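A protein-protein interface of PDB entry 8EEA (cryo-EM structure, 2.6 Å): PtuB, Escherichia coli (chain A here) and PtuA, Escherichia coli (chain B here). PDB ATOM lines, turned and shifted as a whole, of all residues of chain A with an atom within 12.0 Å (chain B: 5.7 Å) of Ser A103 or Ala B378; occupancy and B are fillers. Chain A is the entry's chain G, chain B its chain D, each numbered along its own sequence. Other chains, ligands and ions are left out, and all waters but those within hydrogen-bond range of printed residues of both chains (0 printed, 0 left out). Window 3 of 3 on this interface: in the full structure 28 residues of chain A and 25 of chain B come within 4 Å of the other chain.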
ATOM      1  N   ARG A  64     -16.498   5.473  -4.777  1.00  0.00           N
ATOM      2  CA  ARG A  64     -15.831   5.265  -3.500  1.00  0.00           C
ATOM      3  C   ARG A  64     -14.366   4.880  -3.654  1.00  0.00           C
ATOM      4  O   ARG A  64     -13.665   4.758  -2.646  1.00  0.00           O
ATOM      5  CB  ARG A  64     -16.561   4.185  -2.698  1.00  0.00           C
ATOM      6  CG  ARG A  64     -17.961   4.577  -2.260  1.00  0.00           C
ATOM      7  CD  ARG A  64     -18.715   3.389  -1.694  1.00  0.00           C
ATOM      8  NE  ARG A  64     -20.092   3.724  -1.357  1.00  0.00           N
ATOM      9  CZ  ARG A  64     -20.470   4.297  -0.222  1.00  0.00           C
ATOM     10  NH1 ARG A  64     -19.593   4.619   0.714  1.00  0.00           N
ATOM     11  NH2 ARG A  64     -21.759   4.555  -0.022  1.00  0.00           N
ATOM     12  N   GLY A  65     -13.889   4.689  -4.878  1.00  0.00           N
ATOM     13  CA  GLY A  65     -12.507   4.297  -5.092  1.00  0.00           C
ATOM     14  C   GLY A  65     -12.169   2.917  -4.571  1.00  0.00           C
ATOM     15  O   GLY A  65     -11.109   2.733  -3.962  1.00  0.00           O
ATOM     16  N   LEU A  66     -13.049   1.937  -4.795  1.00  0.00           N
ATOM     17  CA  LEU A  66     -12.812   0.568  -4.360  1.00  0.00           C
ATOM     18  C   LEU A  66     -12.631  -0.415  -5.508  1.00  0.00           C
ATOM     19  O   LEU A  66     -12.087  -1.500  -5.284  1.00  0.00           O
ATOM     20  CB  LEU A  66     -13.969   0.087  -3.472  1.00  0.00           C
ATOM     21  CG  LEU A  66     -14.072   0.779  -2.109  1.00  0.00           C
ATOM     22  CD1 LEU A  66     -15.463   0.606  -1.519  1.00  0.00           C
ATOM     23  CD2 LEU A  66     -13.015   0.248  -1.155  1.00  0.00           C
ATOM     24  N   GLY A  67     -13.069  -0.069  -6.717  1.00  0.00           N
ATOM     25  CA  GLY A  67     -12.815  -0.890  -7.881  1.00  0.00           C
ATOM     26  C   GLY A  67     -13.796  -2.037  -8.041  1.00  0.00           C
ATOM     27  O   GLY A  67     -14.742  -2.217  -7.274  1.00  0.00           O
ATOM     28  N   LEU A  94     -14.667  -4.319  -4.684  1.00  0.00           N
ATOM     29  CA  LEU A  94     -13.412  -4.722  -4.049  1.00  0.00           C
ATOM     30  C   LEU A  94     -12.504  -5.450  -5.046  1.00  0.00           C
ATOM     31  O   LEU A  94     -12.257  -6.653  -4.954  1.00  0.00           O
ATOM     32  CB  LEU A  94     -13.683  -5.585  -2.812  1.00  0.00           C
ATOM     33  CG  LEU A  94     -14.756  -5.058  -1.858  1.00  0.00           C
ATOM     34  CD1 LEU A  94     -14.771  -5.867  -0.575  1.00  0.00           C
ATOM     35  CD2 LEU A  94     -14.538  -3.583  -1.557  1.00  0.00           C
ATOM     36  N   ASP A  95     -12.035  -4.673  -6.022  1.00  0.00           N
ATOM     37  CA  ASP A  95     -11.157  -5.202  -7.061  1.00  0.00           C
ATOM     38  C   ASP A  95     -10.049  -6.060  -6.460  1.00  0.00           C
ATOM     39  O   ASP A  95      -9.517  -5.770  -5.385  1.00  0.00           O
ATOM     40  CB  ASP A  95     -10.545  -4.061  -7.875  1.00  0.00           C
ATOM     41  CG  ASP A  95      -9.657  -3.160  -7.045  1.00  0.00           C
ATOM     42  OD1 ASP A  95      -9.711  -3.249  -5.801  1.00  0.00           O
ATOM     43  OD2 ASP A  95      -8.901  -2.362  -7.637  1.00  0.00           O
ATOM     44  N   SER A  96      -9.702  -7.132  -7.177  1.00  0.00           N
ATOM     45  CA  SER A  96      -8.681  -8.055  -6.691  1.00  0.00           C
ATOM     46  C   SER A  96      -7.298  -7.416  -6.713  1.00  0.00           C
ATOM     47  O   SER A  96      -6.535  -7.539  -5.747  1.00  0.00           O
ATOM     48  CB  SER A  96      -8.691  -9.328  -7.535  1.00  0.00           C
ATOM     49  OG  SER A  96      -8.510  -9.027  -8.907  1.00  0.00           O
ATOM     50  N   GLY A  97      -6.954  -6.738  -7.803  1.00  0.00           N
ATOM     51  CA  GLY A  97      -5.656  -6.104  -7.929  1.00  0.00           C
ATOM     52  C   GLY A  97      -5.432  -5.508  -9.304  1.00  0.00           C
ATOM     53  O   GLY A  97      -6.313  -4.849  -9.857  1.00  0.00           O
ATOM     54  N   SER A 103      -4.964  -0.439   1.245  1.00  0.00           N
ATOM     55  CA  SER A 103      -4.721  -1.663   1.999  1.00  0.00           C
ATOM     56  C   SER A 103      -6.027  -2.380   2.327  1.00  0.00           C
ATOM     57  O   SER A 103      -6.016  -3.518   2.795  1.00  0.00           O
ATOM     58  CB  SER A 103      -3.958  -1.353   3.288  1.00  0.00           C
ATOM     59  OG  SER A 103      -2.794  -0.589   3.022  1.00  0.00           O
ATOM     60  N   SER A 104      -7.151  -1.713   2.079  1.00  0.00           N
ATOM     61  CA  SER A 104      -8.464  -2.298   2.335  1.00  0.00           C
ATOM     62  C   SER A 104      -8.802  -3.280   1.220  1.00  0.00           C
ATOM     63  O   SER A 104      -9.075  -2.874   0.086  1.00  0.00           O
ATOM     64  CB  SER A 104      -9.517  -1.200   2.434  1.00  0.00           C
ATOM     65  OG  SER A 104      -9.654  -0.512   1.204  1.00  0.00           O
ATOM     66  N   LEU A 105      -8.791  -4.570   1.539  1.00  0.00           N
ATOM     67  CA  LEU A 105      -9.015  -5.604   0.539  1.00  0.00           C
ATOM     68  C   LEU A 105      -9.495  -6.865   1.255  1.00  0.00           C
ATOM     69  O   LEU A 105      -9.942  -6.803   2.407  1.00  0.00           O
ATOM     70  CB  LEU A 105      -7.740  -5.816  -0.299  1.00  0.00           C
ATOM     71  CG  LEU A 105      -6.452  -6.196   0.438  1.00  0.00           C
ATOM     72  CD1 LEU A 105      -6.357  -7.701   0.662  1.00  0.00           C
ATOM     73  CD2 LEU A 105      -5.242  -5.687  -0.332  1.00  0.00           C
ATOM     74  N   LYS A 106      -9.424  -8.004   0.564  1.00  0.00           N
ATOM     75  CA  LYS A 106      -9.964  -9.257   1.079  1.00  0.00           C
ATOM     76  C   LYS A 106      -9.593  -9.470   2.540  1.00  0.00           C
ATOM     77  O   LYS A 106      -8.448  -9.264   2.948  1.00  0.00           O
ATOM     78  CB  LYS A 106      -9.453 -10.426   0.235  1.00  0.00           C
ATOM     79  CG  LYS A 106     -10.194 -11.732   0.475  1.00  0.00           C
ATOM     80  CD  LYS A 106      -9.623 -12.869  -0.358  1.00  0.00           C
ATOM     81  CE  LYS A 106      -9.965 -12.725  -1.836  1.00  0.00           C
ATOM     82  NZ  LYS A 106      -8.968 -13.405  -2.707  1.00  0.00           N
ATOM     83  N   GLY A 107     -10.578  -9.894   3.324  1.00  0.00           N
ATOM     84  CA  GLY A 107     -10.360 -10.134   4.737  1.00  0.00           C
ATOM     85  C   GLY A 107     -11.578 -10.786   5.353  1.00  0.00           C
ATOM     86  O   GLY A 107     -12.458 -11.289   4.652  1.00  0.00           O
ATOM     87  N   LYS A 108     -11.615 -10.776   6.686  1.00  0.00           N
ATOM     88  CA  LYS A 108     -12.746 -11.367   7.395  1.00  0.00           C
ATOM     89  C   LYS A 108     -14.043 -10.638   7.074  1.00  0.00           C
ATOM     90  O   LYS A 108     -15.096 -11.266   6.915  1.00  0.00           O
ATOM     91  CB  LYS A 108     -12.492 -11.348   8.902  1.00  0.00           C
ATOM     92  CG  LYS A 108     -11.621 -12.482   9.408  1.00  0.00           C
ATOM     93  CD  LYS A 108     -11.098 -12.189  10.807  1.00  0.00           C
ATOM     94  CE  LYS A 108     -10.572 -13.444  11.486  1.00  0.00           C
ATOM     95  NZ  LYS A 108      -9.871 -14.348  10.534  1.00  0.00           N
ATOM     96  N   ASN A 109     -13.989  -9.313   6.975  1.00  0.00           N
ATOM     97  CA  ASN A 109     -15.176  -8.487   6.801  1.00  0.00           C
ATOM     98  C   ASN A 109     -15.539  -8.266   5.338  1.00  0.00           C
ATOM     99  O   ASN A 109     -16.426  -7.457   5.052  1.00  0.00           O
ATOM    100  CB  ASN A 109     -14.973  -7.137   7.490  1.00  0.00           C
ATOM    101  CG  ASN A 109     -14.402  -7.275   8.884  1.00  0.00           C
ATOM    102  OD1 ASN A 109     -14.511  -8.329   9.509  1.00  0.00           O
ATOM    103  ND2 ASN A 109     -13.785  -6.209   9.378  1.00  0.00           N
ATOM    104  N   ALA A 110     -14.880  -8.956   4.413  1.00  0.00           N
ATOM    105  CA  ALA A 110     -15.182  -8.777   2.999  1.00  0.00           C
ATOM    106  C   ALA A 110     -16.603  -9.241   2.695  1.00  0.00           C
ATOM    107  O   ALA A 110     -17.139 -10.144   3.340  1.00  0.00           O
ATOM    108  CB  ALA A 110     -14.180  -9.547   2.140  1.00  0.00           C
ATOM    109  N   HIS A 114     -15.882 -11.545  -2.487  1.00  0.00           N
ATOM    110  CA  HIS A 114     -14.747 -11.735  -1.596  1.00  0.00           C
ATOM    111  C   HIS A 114     -15.157 -12.175  -0.197  1.00  0.00           C
ATOM    112  O   HIS A 114     -14.293 -12.282   0.679  1.00  0.00           O
ATOM    113  CB  HIS A 114     -13.932 -10.441  -1.508  1.00  0.00           C
ATOM    114  CG  HIS A 114     -13.007 -10.226  -2.666  1.00  0.00           C
ATOM    115  ND1 HIS A 114     -12.529 -11.261  -3.440  1.00  0.00           N
ATOM    116  CD2 HIS A 114     -12.475  -9.094  -3.184  1.00  0.00           C
ATOM    117  CE1 HIS A 114     -11.741 -10.776  -4.383  1.00  0.00           C
ATOM    118  NE2 HIS A 114     -11.692  -9.463  -4.249  1.00  0.00           N
ATOM    119  N   LEU B  17       3.543 -11.388   8.145  1.00  0.00           N
ATOM    120  CA  LEU B  17       2.805 -10.133   8.149  1.00  0.00           C
ATOM    121  C   LEU B  17       3.584  -9.090   7.366  1.00  0.00           C
ATOM    122  O   LEU B  17       4.817  -9.081   7.391  1.00  0.00           O
ATOM    123  CB  LEU B  17       2.554  -9.646   9.584  1.00  0.00           C
ATOM    124  CG  LEU B  17       1.865  -8.289   9.753  1.00  0.00           C
ATOM    125  CD1 LEU B  17       0.382  -8.396   9.473  1.00  0.00           C
ATOM    126  CD2 LEU B  17       2.101  -7.745  11.148  1.00  0.00           C
ATOM    127  N   ASP B  18       2.856  -8.220   6.669  1.00  0.00           N
ATOM    128  CA  ASP B  18       3.418  -7.053   6.000  1.00  0.00           C
ATOM    129  C   ASP B  18       2.575  -5.845   6.368  1.00  0.00           C
ATOM    130  O   ASP B  18       1.348  -5.884   6.239  1.00  0.00           O
ATOM    131  CB  ASP B  18       3.444  -7.233   4.480  1.00  0.00           C
ATOM    132  CG  ASP B  18       4.444  -8.278   4.029  1.00  0.00           C
ATOM    133  OD1 ASP B  18       5.657  -7.987   4.040  1.00  0.00           O
ATOM    134  OD2 ASP B  18       4.014  -9.389   3.659  1.00  0.00           O
ATOM    135  N   ILE B  19       3.222  -4.778   6.827  1.00  0.00           N
ATOM    136  CA  ILE B  19       2.520  -3.579   7.273  1.00  0.00           C
ATOM    137  C   ILE B  19       3.335  -2.353   6.887  1.00  0.00           C
ATOM    138  O   ILE B  19       4.527  -2.269   7.194  1.00  0.00           O
ATOM    139  CB  ILE B  19       2.260  -3.599   8.793  1.00  0.00           C
ATOM    140  CG1 ILE B  19       1.511  -2.334   9.219  1.00  0.00           C
ATOM    141  CG2 ILE B  19       3.560  -3.735   9.566  1.00  0.00           C
ATOM    142  CD1 ILE B  19       0.874  -2.434  10.578  1.00  0.00           C
ATOM    143  N   THR B  20       2.691  -1.405   6.214  1.00  0.00           N
ATOM    144  CA  THR B  20       3.285  -0.118   5.891  1.00  0.00           C
ATOM    145  C   THR B  20       2.810   0.934   6.886  1.00  0.00           C
ATOM    146  O   THR B  20       1.776   0.783   7.539  1.00  0.00           O
ATOM    147  CB  THR B  20       2.928   0.309   4.464  1.00  0.00           C
ATOM    148  OG1 THR B  20       1.506   0.417   4.333  1.00  0.00           O
ATOM    149  CG2 THR B  20       3.447  -0.702   3.458  1.00  0.00           C
ATOM    150  N   ARG B 366      -4.722   1.187  10.538  1.00  0.00           N
ATOM    151  CA  ARG B 366      -4.401  -0.184  10.158  1.00  0.00           C
ATOM    152  C   ARG B 366      -5.191  -1.122  11.058  1.00  0.00           C
ATOM    153  O   ARG B 366      -5.098  -1.032  12.285  1.00  0.00           O
ATOM    154  CB  ARG B 366      -2.901  -0.457  10.271  1.00  0.00           C
ATOM    155  CG  ARG B 366      -2.039   0.387   9.347  1.00  0.00           C
ATOM    156  CD  ARG B 366      -2.247   0.029   7.886  1.00  0.00           C
ATOM    157  NE  ARG B 366      -1.413   0.839   7.006  1.00  0.00           N
ATOM    158  CZ  ARG B 366      -1.705   2.072   6.615  1.00  0.00           C
ATOM    159  NH1 ARG B 366      -2.821   2.671   6.991  1.00  0.00           N
ATOM    160  NH2 ARG B 366      -0.855   2.722   5.826  1.00  0.00           N
ATOM    161  N   LEU B 367      -5.962  -2.020  10.454  1.00  0.00           N
ATOM    162  CA  LEU B 367      -6.728  -3.015  11.193  1.00  0.00           C
ATOM    163  C   LEU B 367      -6.028  -4.362  11.079  1.00  0.00           C
ATOM    164  O   LEU B 367      -5.783  -4.845   9.968  1.00  0.00           O
ATOM    165  CB  LEU B 367      -8.156  -3.104  10.657  1.00  0.00           C
ATOM    166  CG  LEU B 367      -9.000  -1.836  10.789  1.00  0.00           C
ATOM    167  CD1 LEU B 367      -9.936  -1.695   9.606  1.00  0.00           C
ATOM    168  CD2 LEU B 367      -9.782  -1.856  12.086  1.00  0.00           C
ATOM    169  N   LEU B 368      -5.716  -4.968  12.220  1.00  0.00           N
ATOM    170  CA  LEU B 368      -4.967  -6.215  12.268  1.00  0.00           C
ATOM    171  C   LEU B 368      -5.905  -7.390  12.506  1.00  0.00           C
ATOM    172  O   LEU B 368      -6.824  -7.310  13.324  1.00  0.00           O
ATOM    173  CB  LEU B 368      -3.907  -6.174  13.368  1.00  0.00           C
ATOM    174  CG  LEU B 368      -2.860  -5.064  13.274  1.00  0.00           C
ATOM    175  CD1 LEU B 368      -1.961  -5.089  14.491  1.00  0.00           C
ATOM    176  CD2 LEU B 368      -2.041  -5.200  12.006  1.00  0.00           C
ATOM    177  N   GLU B 369      -5.664  -8.483  11.785  1.00  0.00           N
ATOM    178  CA  GLU B 369      -6.427  -9.707  11.959  1.00  0.00           C
ATOM    179  C   GLU B 369      -5.550 -10.900  11.612  1.00  0.00           C
ATOM    180  O   GLU B 369      -4.542 -10.775  10.915  1.00  0.00           O
ATOM    181  CB  GLU B 369      -7.698  -9.718  11.096  1.00  0.00           C
ATOM    182  CG  GLU B 369      -7.451  -9.713   9.588  1.00  0.00           C
ATOM    183  CD  GLU B 369      -7.763  -8.379   8.936  1.00  0.00           C
ATOM    184  OE1 GLU B 369      -7.955  -7.379   9.658  1.00  0.00           O
ATOM    185  OE2 GLU B 369      -7.815  -8.331   7.691  1.00  0.00           O
ATOM    186  N   GLY B 376      -1.265 -13.022   8.991  1.00  0.00           N
ATOM    187  CA  GLY B 376      -1.764 -11.734   9.438  1.00  0.00           C
ATOM    188  C   GLY B 376      -2.012 -10.785   8.282  1.00  0.00           C
ATOM    189  O   GLY B 376      -1.408 -10.913   7.215  1.00  0.00           O
ATOM    190  N   LYS B 377      -2.916  -9.831   8.503  1.00  0.00           N
ATOM    191  CA  LYS B 377      -3.236  -8.801   7.525  1.00  0.00           C
ATOM    192  C   LYS B 377      -3.383  -7.466   8.237  1.00  0.00           C
ATOM    193  O   LYS B 377      -3.897  -7.408   9.356  1.00  0.00           O
ATOM    194  CB  LYS B 377      -4.527  -9.125   6.768  1.00  0.00           C
ATOM    195  CG  LYS B 377      -4.380 -10.198   5.712  1.00  0.00           C
ATOM    196  CD  LYS B 377      -5.712 -10.493   5.047  1.00  0.00           C
ATOM    197  CE  LYS B 377      -5.586 -11.598   4.018  1.00  0.00           C
ATOM    198  NZ  LYS B 377      -4.755 -11.177   2.859  1.00  0.00           N
ATOM    199  N   ALA B 378      -2.936  -6.396   7.583  1.00  0.00           N
ATOM    200  CA  ALA B 378      -3.051  -5.036   8.106  1.00  0.00           C
ATOM    201  C   ALA B 378      -3.710  -4.179   7.029  1.00  0.00           C
ATOM    202  O   ALA B 378      -3.028  -3.651   6.146  1.00  0.00           O
ATOM    203  CB  ALA B 378      -1.690  -4.481   8.505  1.00  0.00           C
ATOM    204  N   LEU B 379      -5.029  -4.035   7.108  1.00  0.00           N
ATOM    205  CA  LEU B 379      -5.823  -3.399   6.069  1.00  0.00           C
ATOM    206  C   LEU B 379      -6.295  -2.021   6.516  1.00  0.00           C
ATOM    207  O   LEU B 379      -6.160  -1.632   7.677  1.00  0.00           O
ATOM    208  CB  LEU B 379      -7.030  -4.270   5.703  1.00  0.00           C
ATOM    209  CG  LEU B 379      -6.773  -5.767   5.531  1.00  0.00           C
ATOM    210  CD1 LEU B 379      -8.089  -6.513   5.437  1.00  0.00           C
ATOM    211  CD2 LEU B 379      -5.918  -6.033   4.308  1.00  0.00           C
ATOM    212  N   MET B 380      -6.860  -1.285   5.562  1.00  0.00           N
ATOM    213  CA  MET B 380      -7.472   0.014   5.782  1.00  0.00           C
ATOM    214  C   MET B 380      -8.979  -0.127   5.926  1.00  0.00           C
ATOM    215  O   MET B 380      -9.573  -1.095   5.446  1.00  0.00           O
ATOM    216  CB  MET B 380      -7.166   0.953   4.610  1.00  0.00           C
ATOM    217  CG  MET B 380      -5.867   1.720   4.730  1.00  0.00           C
ATOM    218  SD  MET B 380      -5.510   2.656   3.230  1.00  0.00           S
ATOM    219  CE  MET B 380      -3.741   2.884   3.376  1.00  0.00           C
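N of Ser A103 sits at hydrogen-bond distance from SD of Met B380 (3.7 Å).
The backbone NH of Lys B377 lies within hydrogen-bond range of the backbone carbonyl oxygen of Glu B369 (3.1 Å).
The backbone NH of Leu B367 lies within hydrogen-bond range of the backbone carbonyl oxygen of Leu B379, 2.8 Å away.
Among the printed residues, pairs that only touch across the chains: Ser A103 with Leu B379, Ser A104 with Met B380, Leu A105 with Leu B379, Lys A106 with Lys B377, Lys A106 with Leu B379 and Ser A103 with Ala B378.
Of chain B, only Ala B378, Leu B379 and Met B380 come within 4 Å of Ser A103.
Printed residues of chain A within 4 Å of Ala B378: Ser A103.
No residue of chain A comes within 4 Å of Thr B20.
No residue of chain A comes within 4 Å of Arg B366.
No residue of chain A comes within 4 Å of Leu B368.
No residue of chain A comes within 4 Å of Glu B369.
No residue of chain A comes within 4 Å of Gly B376.
Lys B377 touches just one residue of chain A: Lys A106 (3.7 Å).
Of chain A, only Ser A103, Leu A105 and Lys A106 come within 4 Å of Leu B379.
Of the printed residues of chain B, Ser A104 touches Met B380.
Printed residues of chain B within 4 Å of Leu A105: Leu B379 (3.6 Å).
The nearest residue of chain B that does not touch Ser A103 is Arg B366 (4.5 Å).
Hydrophobic or aromatic side chains of chain B within 4 Å of the printed part of chain A: Leu B379 and Met B380.
Printed residues of chain A that touch a printed residue of chain B: Ser A103, Ser A104, Leu A105 and Lys A106.
Among the printed residues, 7 pairs touch across the chains.
Among the printed residues, no Asp or Glu carboxylate lies within 4 Å of a Lys or Arg side-chain nitrogen of the other chain.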
